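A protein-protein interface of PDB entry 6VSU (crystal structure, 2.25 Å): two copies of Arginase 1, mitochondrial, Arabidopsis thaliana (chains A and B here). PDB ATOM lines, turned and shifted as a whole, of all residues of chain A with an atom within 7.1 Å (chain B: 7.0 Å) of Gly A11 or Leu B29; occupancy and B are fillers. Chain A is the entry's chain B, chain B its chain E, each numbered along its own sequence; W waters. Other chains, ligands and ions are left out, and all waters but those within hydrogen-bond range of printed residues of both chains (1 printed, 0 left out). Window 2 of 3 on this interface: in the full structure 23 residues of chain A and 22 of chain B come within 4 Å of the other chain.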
ATOM      1  N   SER A   6       6.679  23.157 -25.465  1.00  0.00           N
ATOM      2  CA  SER A   6       5.587  23.647 -26.356  1.00  0.00           C
ATOM      3  C   SER A   6       4.945  22.457 -27.087  1.00  0.00           C
ATOM      4  O   SER A   6       4.056  22.695 -27.931  1.00  0.00           O
ATOM      5  CB  SER A   6       6.117  24.686 -27.332  1.00  0.00           C
ATOM      6  OG  SER A   6       5.104  25.619 -27.681  1.00  0.00           O
ATOM      7  N   SER A   7       5.385  21.228 -26.783  1.00  0.00           N
ATOM      8  CA  SER A   7       4.640  19.970 -27.075  1.00  0.00           C
ATOM      9  C   SER A   7       3.221  20.049 -26.472  1.00  0.00           C
ATOM     10  O   SER A   7       2.305  19.305 -26.936  1.00  0.00           O
ATOM     11  CB  SER A   7       5.402  18.774 -26.548  1.00  0.00           C
ATOM     12  OG  SER A   7       4.690  17.573 -26.771  1.00  0.00           O
ATOM     13  N   ILE A   8       3.036  20.894 -25.448  1.00  0.00           N
ATOM     14  CA  ILE A   8       1.733  21.022 -24.734  1.00  0.00           C
ATOM     15  C   ILE A   8       0.804  21.852 -25.627  1.00  0.00           C
ATOM     16  O   ILE A   8      -0.306  21.356 -25.969  1.00  0.00           O
ATOM     17  CB  ILE A   8       1.887  21.607 -23.309  1.00  0.00           C
ATOM     18  CG1 ILE A   8       2.530  20.597 -22.344  1.00  0.00           C
ATOM     19  CG2 ILE A   8       0.544  22.121 -22.778  1.00  0.00           C
ATOM     20  CD1 ILE A   8       1.689  19.356 -22.002  1.00  0.00           C
ATOM     21  N   GLU A   9       1.241  23.061 -25.983  1.00  0.00           N
ATOM     22  CA  GLU A   9       0.370  24.002 -26.729  1.00  0.00           C
ATOM     23  C   GLU A   9       0.031  23.408 -28.108  1.00  0.00           C
ATOM     24  O   GLU A   9      -1.120  23.578 -28.550  1.00  0.00           O
ATOM     25  CB  GLU A   9       0.993  25.386 -26.854  1.00  0.00           C
ATOM     26  CG  GLU A   9      -0.060  26.425 -27.188  1.00  0.00           C
ATOM     27  CD  GLU A   9       0.389  27.871 -27.093  1.00  0.00           C
ATOM     28  OE1 GLU A   9       1.578  28.091 -26.735  1.00  0.00           O
ATOM     29  OE2 GLU A   9      -0.445  28.774 -27.379  1.00  0.00           O
ATOM     30  N   LYS A  10       0.979  22.718 -28.740  1.00  0.00           N
ATOM     31  CA  LYS A  10       0.804  22.098 -30.078  1.00  0.00           C
ATOM     32  C   LYS A  10      -0.206  20.942 -29.999  1.00  0.00           C
ATOM     33  O   LYS A  10      -0.968  20.800 -30.958  1.00  0.00           O
ATOM     34  CB  LYS A  10       2.153  21.639 -30.652  1.00  0.00           C
ATOM     35  CG  LYS A  10       2.264  21.847 -32.156  1.00  0.00           C
ATOM     36  CD  LYS A  10       3.655  21.895 -32.745  1.00  0.00           C
ATOM     37  CE  LYS A  10       3.568  21.904 -34.262  1.00  0.00           C
ATOM     38  NZ  LYS A  10       4.888  21.864 -34.930  1.00  0.00           N
ATOM     39  N   GLY A  11      -0.185  20.138 -28.923  1.00  0.00           N
ATOM     40  CA  GLY A  11      -1.149  19.052 -28.665  1.00  0.00           C
ATOM     41  C   GLY A  11      -2.556  19.607 -28.484  1.00  0.00           C
ATOM     42  O   GLY A  11      -3.527  19.050 -29.102  1.00  0.00           O
ATOM     43  N   GLN A  12      -2.660  20.703 -27.717  1.00  0.00           N
ATOM     44  CA  GLN A  12      -3.918  21.440 -27.488  1.00  0.00           C
ATOM     45  C   GLN A  12      -4.462  21.855 -28.845  1.00  0.00           C
ATOM     46  O   GLN A  12      -5.686  21.747 -29.085  1.00  0.00           O
ATOM     47  CB  GLN A  12      -3.656  22.643 -26.598  1.00  0.00           C
ATOM     48  CG  GLN A  12      -3.418  22.227 -25.162  1.00  0.00           C
ATOM     49  CD  GLN A  12      -3.091  23.368 -24.238  1.00  0.00           C
ATOM     50  OE1 GLN A  12      -2.974  24.502 -24.645  1.00  0.00           O
ATOM     51  NE2 GLN A  12      -2.959  23.086 -22.966  1.00  0.00           N
ATOM     52  N   ASN A  13      -3.560  22.317 -29.706  1.00  0.00           N
ATOM     53  CA  ASN A  13      -3.911  22.896 -31.025  1.00  0.00           C
ATOM     54  C   ASN A  13      -4.546  21.801 -31.878  1.00  0.00           C
ATOM     55  O   ASN A  13      -5.455  22.122 -32.644  1.00  0.00           O
ATOM     56  CB  ASN A  13      -2.698  23.560 -31.688  1.00  0.00           C
ATOM     57  CG  ASN A  13      -2.398  24.934 -31.120  1.00  0.00           C
ATOM     58  OD1 ASN A  13      -3.255  25.578 -30.509  1.00  0.00           O
ATOM     59  ND2 ASN A  13      -1.193  25.415 -31.369  1.00  0.00           N
ATOM     60  N   ARG A  14      -4.067  20.563 -31.750  1.00  0.00           N
ATOM     61  CA  ARG A  14      -4.549  19.445 -32.594  1.00  0.00           C
ATOM     62  C   ARG A  14      -6.002  19.142 -32.194  1.00  0.00           C
ATOM     63  O   ARG A  14      -6.841  18.861 -33.096  1.00  0.00           O
ATOM     64  CB  ARG A  14      -3.601  18.246 -32.495  1.00  0.00           C
ATOM     65  CG  ARG A  14      -2.179  18.563 -32.930  1.00  0.00           C
ATOM     66  CD  ARG A  14      -1.567  17.548 -33.862  1.00  0.00           C
ATOM     67  NE  ARG A  14      -2.218  17.340 -35.197  1.00  0.00           N
ATOM     68  CZ  ARG A  14      -1.622  17.463 -36.436  1.00  0.00           C
ATOM     69  NH1 ARG A  14      -0.361  17.868 -36.586  1.00  0.00           N
ATOM     70  NH2 ARG A  14      -2.309  17.172 -37.536  1.00  0.00           N
ATOM     71  N   VAL A  15      -6.287  19.268 -30.899  1.00  0.00           N
ATOM     72  CA  VAL A  15      -7.642  19.036 -30.327  1.00  0.00           C
ATOM     73  C   VAL A  15      -8.575  20.170 -30.765  1.00  0.00           C
ATOM     74  O   VAL A  15      -9.724  19.873 -31.138  1.00  0.00           O
ATOM     75  CB  VAL A  15      -7.599  18.889 -28.804  1.00  0.00           C
ATOM     76  CG1 VAL A  15      -8.998  18.958 -28.217  1.00  0.00           C
ATOM     77  CG2 VAL A  15      -6.921  17.584 -28.428  1.00  0.00           C
ATOM     78  N   ILE A  16      -8.092  21.414 -30.679  1.00  0.00           N
ATOM     79  CA  ILE A  16      -8.863  22.619 -31.111  1.00  0.00           C
ATOM     80  C   ILE A  16      -9.168  22.452 -32.609  1.00  0.00           C
ATOM     81  O   ILE A  16     -10.310  22.613 -32.986  1.00  0.00           O
ATOM     82  CB  ILE A  16      -8.069  23.906 -30.802  1.00  0.00           C
ATOM     83  CG1 ILE A  16      -8.035  24.116 -29.290  1.00  0.00           C
ATOM     84  CG2 ILE A  16      -8.644  25.109 -31.571  1.00  0.00           C
ATOM     85  CD1 ILE A  16      -7.190  25.269 -28.812  1.00  0.00           C
ATOM     86  N   ASP A  17      -8.153  22.135 -33.422  1.00  0.00           N
ATOM     87  CA  ASP A  17      -8.308  22.006 -34.889  1.00  0.00           C
ATOM     88  C   ASP A  17      -9.348  20.912 -35.201  1.00  0.00           C
ATOM     89  O   ASP A  17     -10.220  21.168 -36.055  1.00  0.00           O
ATOM     90  CB  ASP A  17      -6.945  21.818 -35.561  1.00  0.00           C
ATOM     91  CG  ASP A  17      -6.111  23.097 -35.475  1.00  0.00           C
ATOM     92  OD1 ASP A  17      -6.654  24.141 -34.987  1.00  0.00           O
ATOM     93  OD2 ASP A  17      -4.918  23.052 -35.864  1.00  0.00           O
ATOM     94  N   ASP A 106     -10.442  20.299 -20.780  1.00  0.00           N
ATOM     95  CA  ASP A 106      -9.809  19.162 -20.065  1.00  0.00           C
ATOM     96  C   ASP A 106      -8.364  18.995 -20.575  1.00  0.00           C
ATOM     97  O   ASP A 106      -7.607  18.339 -19.924  1.00  0.00           O
ATOM     98  CB  ASP A 106     -10.626  17.873 -20.188  1.00  0.00           C
ATOM     99  CG  ASP A 106     -10.310  16.887 -19.070  1.00  0.00           C
ATOM    100  OD1 ASP A 106     -10.522  17.265 -17.889  1.00  0.00           O
ATOM    101  OD2 ASP A 106      -9.804  15.783 -19.353  1.00  0.00           O
ATOM    102  N   CYS A 107      -7.946  19.583 -21.680  1.00  0.00           N
ATOM    103  CA  CYS A 107      -6.563  19.331 -22.131  1.00  0.00           C
ATOM    104  C   CYS A 107      -5.720  20.581 -21.837  1.00  0.00           C
ATOM    105  O   CYS A 107      -4.611  20.658 -22.326  1.00  0.00           O
ATOM    106  CB  CYS A 107      -6.569  18.836 -23.579  1.00  0.00           C
ATOM    107  SG  CYS A 107      -6.951  20.116 -24.794  1.00  0.00           S
ATOM    108  N   GLY A 108      -6.269  21.517 -21.052  1.00  0.00           N
ATOM    109  CA  GLY A 108      -5.540  22.611 -20.402  1.00  0.00           C
ATOM    110  C   GLY A 108      -5.636  23.900 -21.178  1.00  0.00           C
ATOM    111  O   GLY A 108      -4.936  24.774 -20.818  1.00  0.00           O
ATOM    112  N   VAL A 109      -6.454  24.001 -22.222  1.00  0.00           N
ATOM    113  CA  VAL A 109      -6.607  25.242 -23.031  1.00  0.00           C
ATOM    114  C   VAL A 109      -7.105  26.399 -22.157  1.00  0.00           C
ATOM    115  O   VAL A 109      -8.109  26.244 -21.441  1.00  0.00           O
ATOM    116  CB  VAL A 109      -7.523  24.976 -24.234  1.00  0.00           C
ATOM    117  CG1 VAL A 109      -7.941  26.227 -24.968  1.00  0.00           C
ATOM    118  CG2 VAL A 109      -6.873  24.011 -25.191  1.00  0.00           C
ATOM    119  N   ARG A 113      -8.012  31.313 -25.701  1.00  0.00           N
ATOM    120  CA  ARG A 113      -8.064  30.367 -26.843  1.00  0.00           C
ATOM    121  C   ARG A 113      -9.399  29.644 -26.818  1.00  0.00           C
ATOM    122  O   ARG A 113      -9.922  29.358 -27.869  1.00  0.00           O
ATOM    123  CB  ARG A 113      -6.886  29.399 -26.795  1.00  0.00           C
ATOM    124  CG  ARG A 113      -5.559  30.084 -27.048  1.00  0.00           C
ATOM    125  CD  ARG A 113      -4.427  29.262 -26.482  1.00  0.00           C
ATOM    126  NE  ARG A 113      -4.183  28.029 -27.231  1.00  0.00           N
ATOM    127  CZ  ARG A 113      -3.711  26.927 -26.684  1.00  0.00           C
ATOM    128  NH1 ARG A 113      -3.491  26.893 -25.371  1.00  0.00           N
ATOM    129  NH2 ARG A 113      -3.499  25.855 -27.436  1.00  0.00           N
ATOM    130  N   ARG B  24      -9.324  10.548 -31.158  1.00  0.00           N
ATOM    131  CA  ARG B  24      -7.923  10.071 -31.264  1.00  0.00           C
ATOM    132  C   ARG B  24      -6.963  11.121 -30.700  1.00  0.00           C
ATOM    133  O   ARG B  24      -6.090  10.742 -29.936  1.00  0.00           O
ATOM    134  CB  ARG B  24      -7.565   9.723 -32.711  1.00  0.00           C
ATOM    135  CG  ARG B  24      -6.082   9.470 -32.925  1.00  0.00           C
ATOM    136  CD  ARG B  24      -5.705   8.881 -34.269  1.00  0.00           C
ATOM    137  NE  ARG B  24      -6.790   8.849 -35.229  1.00  0.00           N
ATOM    138  CZ  ARG B  24      -7.084   9.813 -36.084  1.00  0.00           C
ATOM    139  NH1 ARG B  24      -6.361  10.916 -36.118  1.00  0.00           N
ATOM    140  NH2 ARG B  24      -8.108   9.663 -36.896  1.00  0.00           N
ATOM    141  N   GLU B  25      -7.192  12.396 -30.991  1.00  0.00           N
ATOM    142  CA  GLU B  25      -6.247  13.457 -30.557  1.00  0.00           C
ATOM    143  C   GLU B  25      -6.343  13.633 -29.036  1.00  0.00           C
ATOM    144  O   GLU B  25      -5.345  13.900 -28.429  1.00  0.00           O
ATOM    145  CB  GLU B  25      -6.515  14.761 -31.294  1.00  0.00           C
ATOM    146  CG  GLU B  25      -6.393  14.670 -32.790  1.00  0.00           C
ATOM    147  CD  GLU B  25      -4.975  14.510 -33.336  1.00  0.00           C
ATOM    148  OE1 GLU B  25      -3.967  14.461 -32.574  1.00  0.00           O
ATOM    149  OE2 GLU B  25      -4.905  14.385 -34.542  1.00  0.00           O
ATOM    150  N   ARG B  26      -7.551  13.559 -28.473  1.00  0.00           N
ATOM    151  CA  ARG B  26      -7.722  13.688 -27.001  1.00  0.00           C
ATOM    152  C   ARG B  26      -7.030  12.511 -26.300  1.00  0.00           C
ATOM    153  O   ARG B  26      -6.302  12.756 -25.335  1.00  0.00           O
ATOM    154  CB  ARG B  26      -9.204  13.817 -26.633  1.00  0.00           C
ATOM    155  CG  ARG B  26      -9.898  15.023 -27.253  1.00  0.00           C
ATOM    156  CD  ARG B  26     -11.155  15.475 -26.536  1.00  0.00           C
ATOM    157  NE  ARG B  26     -12.202  14.468 -26.492  1.00  0.00           N
ATOM    158  CZ  ARG B  26     -13.406  14.597 -27.027  1.00  0.00           C
ATOM    159  NH1 ARG B  26     -13.748  15.709 -27.645  1.00  0.00           N
ATOM    160  NH2 ARG B  26     -14.276  13.613 -26.933  1.00  0.00           N
ATOM    161  N   ALA B  27      -7.198  11.300 -26.831  1.00  0.00           N
ATOM    162  CA  ALA B  27      -6.596  10.068 -26.284  1.00  0.00           C
ATOM    163  C   ALA B  27      -5.073  10.184 -26.365  1.00  0.00           C
ATOM    164  O   ALA B  27      -4.386   9.789 -25.410  1.00  0.00           O
ATOM    165  CB  ALA B  27      -7.115   8.838 -26.977  1.00  0.00           C
ATOM    166  N   LYS B  28      -4.547  10.748 -27.428  1.00  0.00           N
ATOM    167  CA  LYS B  28      -3.079  10.844 -27.604  1.00  0.00           C
ATOM    168  C   LYS B  28      -2.471  11.702 -26.476  1.00  0.00           C
ATOM    169  O   LYS B  28      -1.480  11.297 -25.910  1.00  0.00           O
ATOM    170  CB  LYS B  28      -2.738  11.387 -28.990  1.00  0.00           C
ATOM    171  CG  LYS B  28      -1.256  11.713 -29.180  1.00  0.00           C
ATOM    172  CD  LYS B  28      -0.783  11.626 -30.613  1.00  0.00           C
ATOM    173  CE  LYS B  28       0.262  12.639 -31.018  1.00  0.00           C
ATOM    174  NZ  LYS B  28       1.350  12.817 -30.033  1.00  0.00           N
ATOM    175  N   LEU B  29      -3.065  12.838 -26.131  1.00  0.00           N
ATOM    176  CA  LEU B  29      -2.587  13.703 -25.010  1.00  0.00           C
ATOM    177  C   LEU B  29      -2.654  12.943 -23.679  1.00  0.00           C
ATOM    178  O   LEU B  29      -1.757  13.135 -22.840  1.00  0.00           O
ATOM    179  CB  LEU B  29      -3.455  14.963 -24.952  1.00  0.00           C
ATOM    180  CG  LEU B  29      -3.410  15.847 -26.197  1.00  0.00           C
ATOM    181  CD1 LEU B  29      -4.041  17.193 -25.919  1.00  0.00           C
ATOM    182  CD2 LEU B  29      -1.981  16.051 -26.647  1.00  0.00           C
ATOM    183  N   LYS B  30      -3.707  12.130 -23.474  1.00  0.00           N
ATOM    184  CA  LYS B  30      -3.905  11.439 -22.187  1.00  0.00           C
ATOM    185  C   LYS B  30      -2.855  10.333 -22.070  1.00  0.00           C
ATOM    186  O   LYS B  30      -2.251  10.249 -20.977  1.00  0.00           O
ATOM    187  CB  LYS B  30      -5.347  10.986 -22.026  1.00  0.00           C
ATOM    188  CG  LYS B  30      -6.395  12.084 -21.886  1.00  0.00           C
ATOM    189  CD  LYS B  30      -5.996  13.313 -21.138  1.00  0.00           C
ATOM    190  CE  LYS B  30      -7.125  14.320 -21.177  1.00  0.00           C
ATOM    191  NZ  LYS B  30      -6.921  15.409 -20.204  1.00  0.00           N
ATOM    192  N   GLY B  31      -2.581   9.595 -23.162  1.00  0.00           N
ATOM    193  CA  GLY B  31      -1.572   8.538 -23.173  1.00  0.00           C
ATOM    194  C   GLY B  31      -0.207   9.128 -22.906  1.00  0.00           C
ATOM    195  O   GLY B  31       0.537   8.532 -22.155  1.00  0.00           O
ATOM    196  N   GLU B  32       0.134  10.245 -23.547  1.00  0.00           N
ATOM    197  CA  GLU B  32       1.441  10.921 -23.379  1.00  0.00           C
ATOM    198  C   GLU B  32       1.579  11.405 -21.943  1.00  0.00           C
ATOM    199  O   GLU B  32       2.624  11.151 -21.330  1.00  0.00           O
ATOM    200  CB  GLU B  32       1.608  12.059 -24.381  1.00  0.00           C
ATOM    201  CG  GLU B  32       1.702  11.550 -25.796  1.00  0.00           C
ATOM    202  CD  GLU B  32       1.799  12.676 -26.802  1.00  0.00           C
ATOM    203  OE1 GLU B  32       2.120  12.383 -27.956  1.00  0.00           O
ATOM    204  OE2 GLU B  32       1.533  13.858 -26.402  1.00  0.00           O
ATOM    205  N   LEU B  33       0.556  12.010 -21.377  1.00  0.00           N
ATOM    206  CA  LEU B  33       0.639  12.409 -19.954  1.00  0.00           C
ATOM    207  C   LEU B  33       0.917  11.189 -19.069  1.00  0.00           C
ATOM    208  O   LEU B  33       1.844  11.223 -18.236  1.00  0.00           O
ATOM    209  CB  LEU B  33      -0.655  13.108 -19.573  1.00  0.00           C
ATOM    210  CG  LEU B  33      -0.829  13.510 -18.107  1.00  0.00           C
ATOM    211  CD1 LEU B  33       0.342  14.346 -17.587  1.00  0.00           C
ATOM    212  CD2 LEU B  33      -2.134  14.315 -17.982  1.00  0.00           C
ATOM    213  N   VAL B  34       0.143  10.128 -19.227  1.00  0.00           N
ATOM    214  CA  VAL B  34       0.332   8.926 -18.374  1.00  0.00           C
ATOM    215  C   VAL B  34       1.753   8.408 -18.531  1.00  0.00           C
ATOM    216  O   VAL B  34       2.359   8.066 -17.512  1.00  0.00           O
ATOM    217  CB  VAL B  34      -0.686   7.833 -18.679  1.00  0.00           C
ATOM    218  CG1 VAL B  34      -0.311   6.562 -17.948  1.00  0.00           C
ATOM    219  CG2 VAL B  34      -2.083   8.296 -18.284  1.00  0.00           C
ATOM    220  N   ARG B  35       2.241   8.325 -19.762  1.00  0.00           N
ATOM    221  CA  ARG B  35       3.561   7.722 -20.040  1.00  0.00           C
ATOM    222  C   ARG B  35       4.651   8.625 -19.478  1.00  0.00           C
ATOM    223  O   ARG B  35       5.681   8.081 -19.047  1.00  0.00           O
ATOM    224  CB  ARG B  35       3.756   7.457 -21.539  1.00  0.00           C
ATOM    225  CG  ARG B  35       2.920   6.290 -22.056  1.00  0.00           C
ATOM    226  CD  ARG B  35       3.263   5.866 -23.475  1.00  0.00           C
ATOM    227  NE  ARG B  35       2.979   6.862 -24.494  1.00  0.00           N
ATOM    228  CZ  ARG B  35       1.817   7.039 -25.108  1.00  0.00           C
ATOM    229  NH1 ARG B  35       0.743   6.311 -24.828  1.00  0.00           N
ATOM    230  NH2 ARG B  35       1.706   7.982 -26.012  1.00  0.00           N
ATOM    231  N   THR B  94      -7.823   9.242 -16.266  1.00  0.00           N
ATOM    232  CA  THR B  94      -7.938  10.345 -17.257  1.00  0.00           C
ATOM    233  C   THR B  94      -9.313  10.233 -17.914  1.00  0.00           C
ATOM    234  O   THR B  94     -10.006   9.291 -17.630  1.00  0.00           O
ATOM    235  CB  THR B  94      -6.818  10.328 -18.315  1.00  0.00           C
ATOM    236  OG1 THR B  94      -6.790   9.049 -18.929  1.00  0.00           O
ATOM    237  CG2 THR B  94      -5.483  10.665 -17.720  1.00  0.00           C
ATOM    238  N   GLU B 128      -3.769   3.713 -27.126  1.00  0.00           N
ATOM    239  CA  GLU B 128      -2.817   4.532 -26.352  1.00  0.00           C
ATOM    240  C   GLU B 128      -2.471   3.797 -25.065  1.00  0.00           C
ATOM    241  O   GLU B 128      -3.181   3.879 -24.092  1.00  0.00           O
ATOM    242  CB  GLU B 128      -3.392   5.924 -26.107  1.00  0.00           C
ATOM    243  CG  GLU B 128      -3.521   6.697 -27.399  1.00  0.00           C
ATOM    244  CD  GLU B 128      -2.202   7.232 -27.917  1.00  0.00           C
ATOM    245  OE1 GLU B 128      -1.205   7.328 -27.143  1.00  0.00           O
ATOM    246  OE2 GLU B 128      -2.193   7.611 -29.069  1.00  0.00           O
ATOM    247  N   LEU B 131      -3.691   2.952 -21.470  1.00  0.00           N
ATOM    248  CA  LEU B 131      -5.068   3.283 -21.134  1.00  0.00           C
ATOM    249  C   LEU B 131      -5.926   2.020 -21.305  1.00  0.00           C
ATOM    250  O   LEU B 131      -5.745   1.279 -22.284  1.00  0.00           O
ATOM    251  CB  LEU B 131      -5.586   4.411 -22.029  1.00  0.00           C
ATOM    252  CG  LEU B 131      -4.794   5.709 -22.069  1.00  0.00           C
ATOM    253  CD1 LEU B 131      -5.532   6.712 -22.949  1.00  0.00           C
ATOM    254  CD2 LEU B 131      -4.490   6.313 -20.714  1.00  0.00           C
HETATM  255  O   HOH W   1      -8.362  13.957 -17.803  1.00  0.00           O
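No position is printed for both chains.
The side-chain carboxylate of Asp A106 lies within salt-bridge range of the side-chain amino group of Lys B30, at 3.0 Å.
The side-chain amide nitrogen (NE2) of Gln A12 sits at hydrogen-bond distance from the backbone carbonyl oxygen (O) of Cys A107 (3.0 Å).
Of chain B, only Leu B29 comes within 4 Å of Gly A11.
Asn A13 touches none of the printed residues of chain B.
Printed residues of chain B within 4 Å of Arg A14: Glu B25.
Printed residues of chain B within 4 Å of Val A15: Leu B29.
Of the printed residues of chain B, Cys A107 touches Leu B29.
Leu B29 touches just these residues of chain A: Gly A11 (3.7 Å), Val A15 (3.8 Å) and Cys A107 (3.8 Å).
Of the printed residues of chain A, Lys B30 touches Asp A106 (3.0 Å).
Arg B35 touches none of the printed residues of chain A.
Water W1 bridges the side-chain carboxylate (OD2) of Asp A106 (2.8 Å) and the side-chain amino group (NZ) of Lys B30 (3.2 Å).
Of the 17 printed residues of chain A, 5 touch a printed residue of chain B.
Hydrophobic or aromatic side chains of chain B within 4 Å of the printed part of chain A: Leu B29.
Among the printed residues, 5 pairs touch across the chains.
CA of Gly A11 touches CD2 of Leu B29, 3.7 Å away.
CB of Arg A14 touches OE1 of Glu B25, 3.8 Å away.
CD1 of Leu B29 touches CG2 of Val A15, at 3.8 Å.
Cys A107 touches Leu B29.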
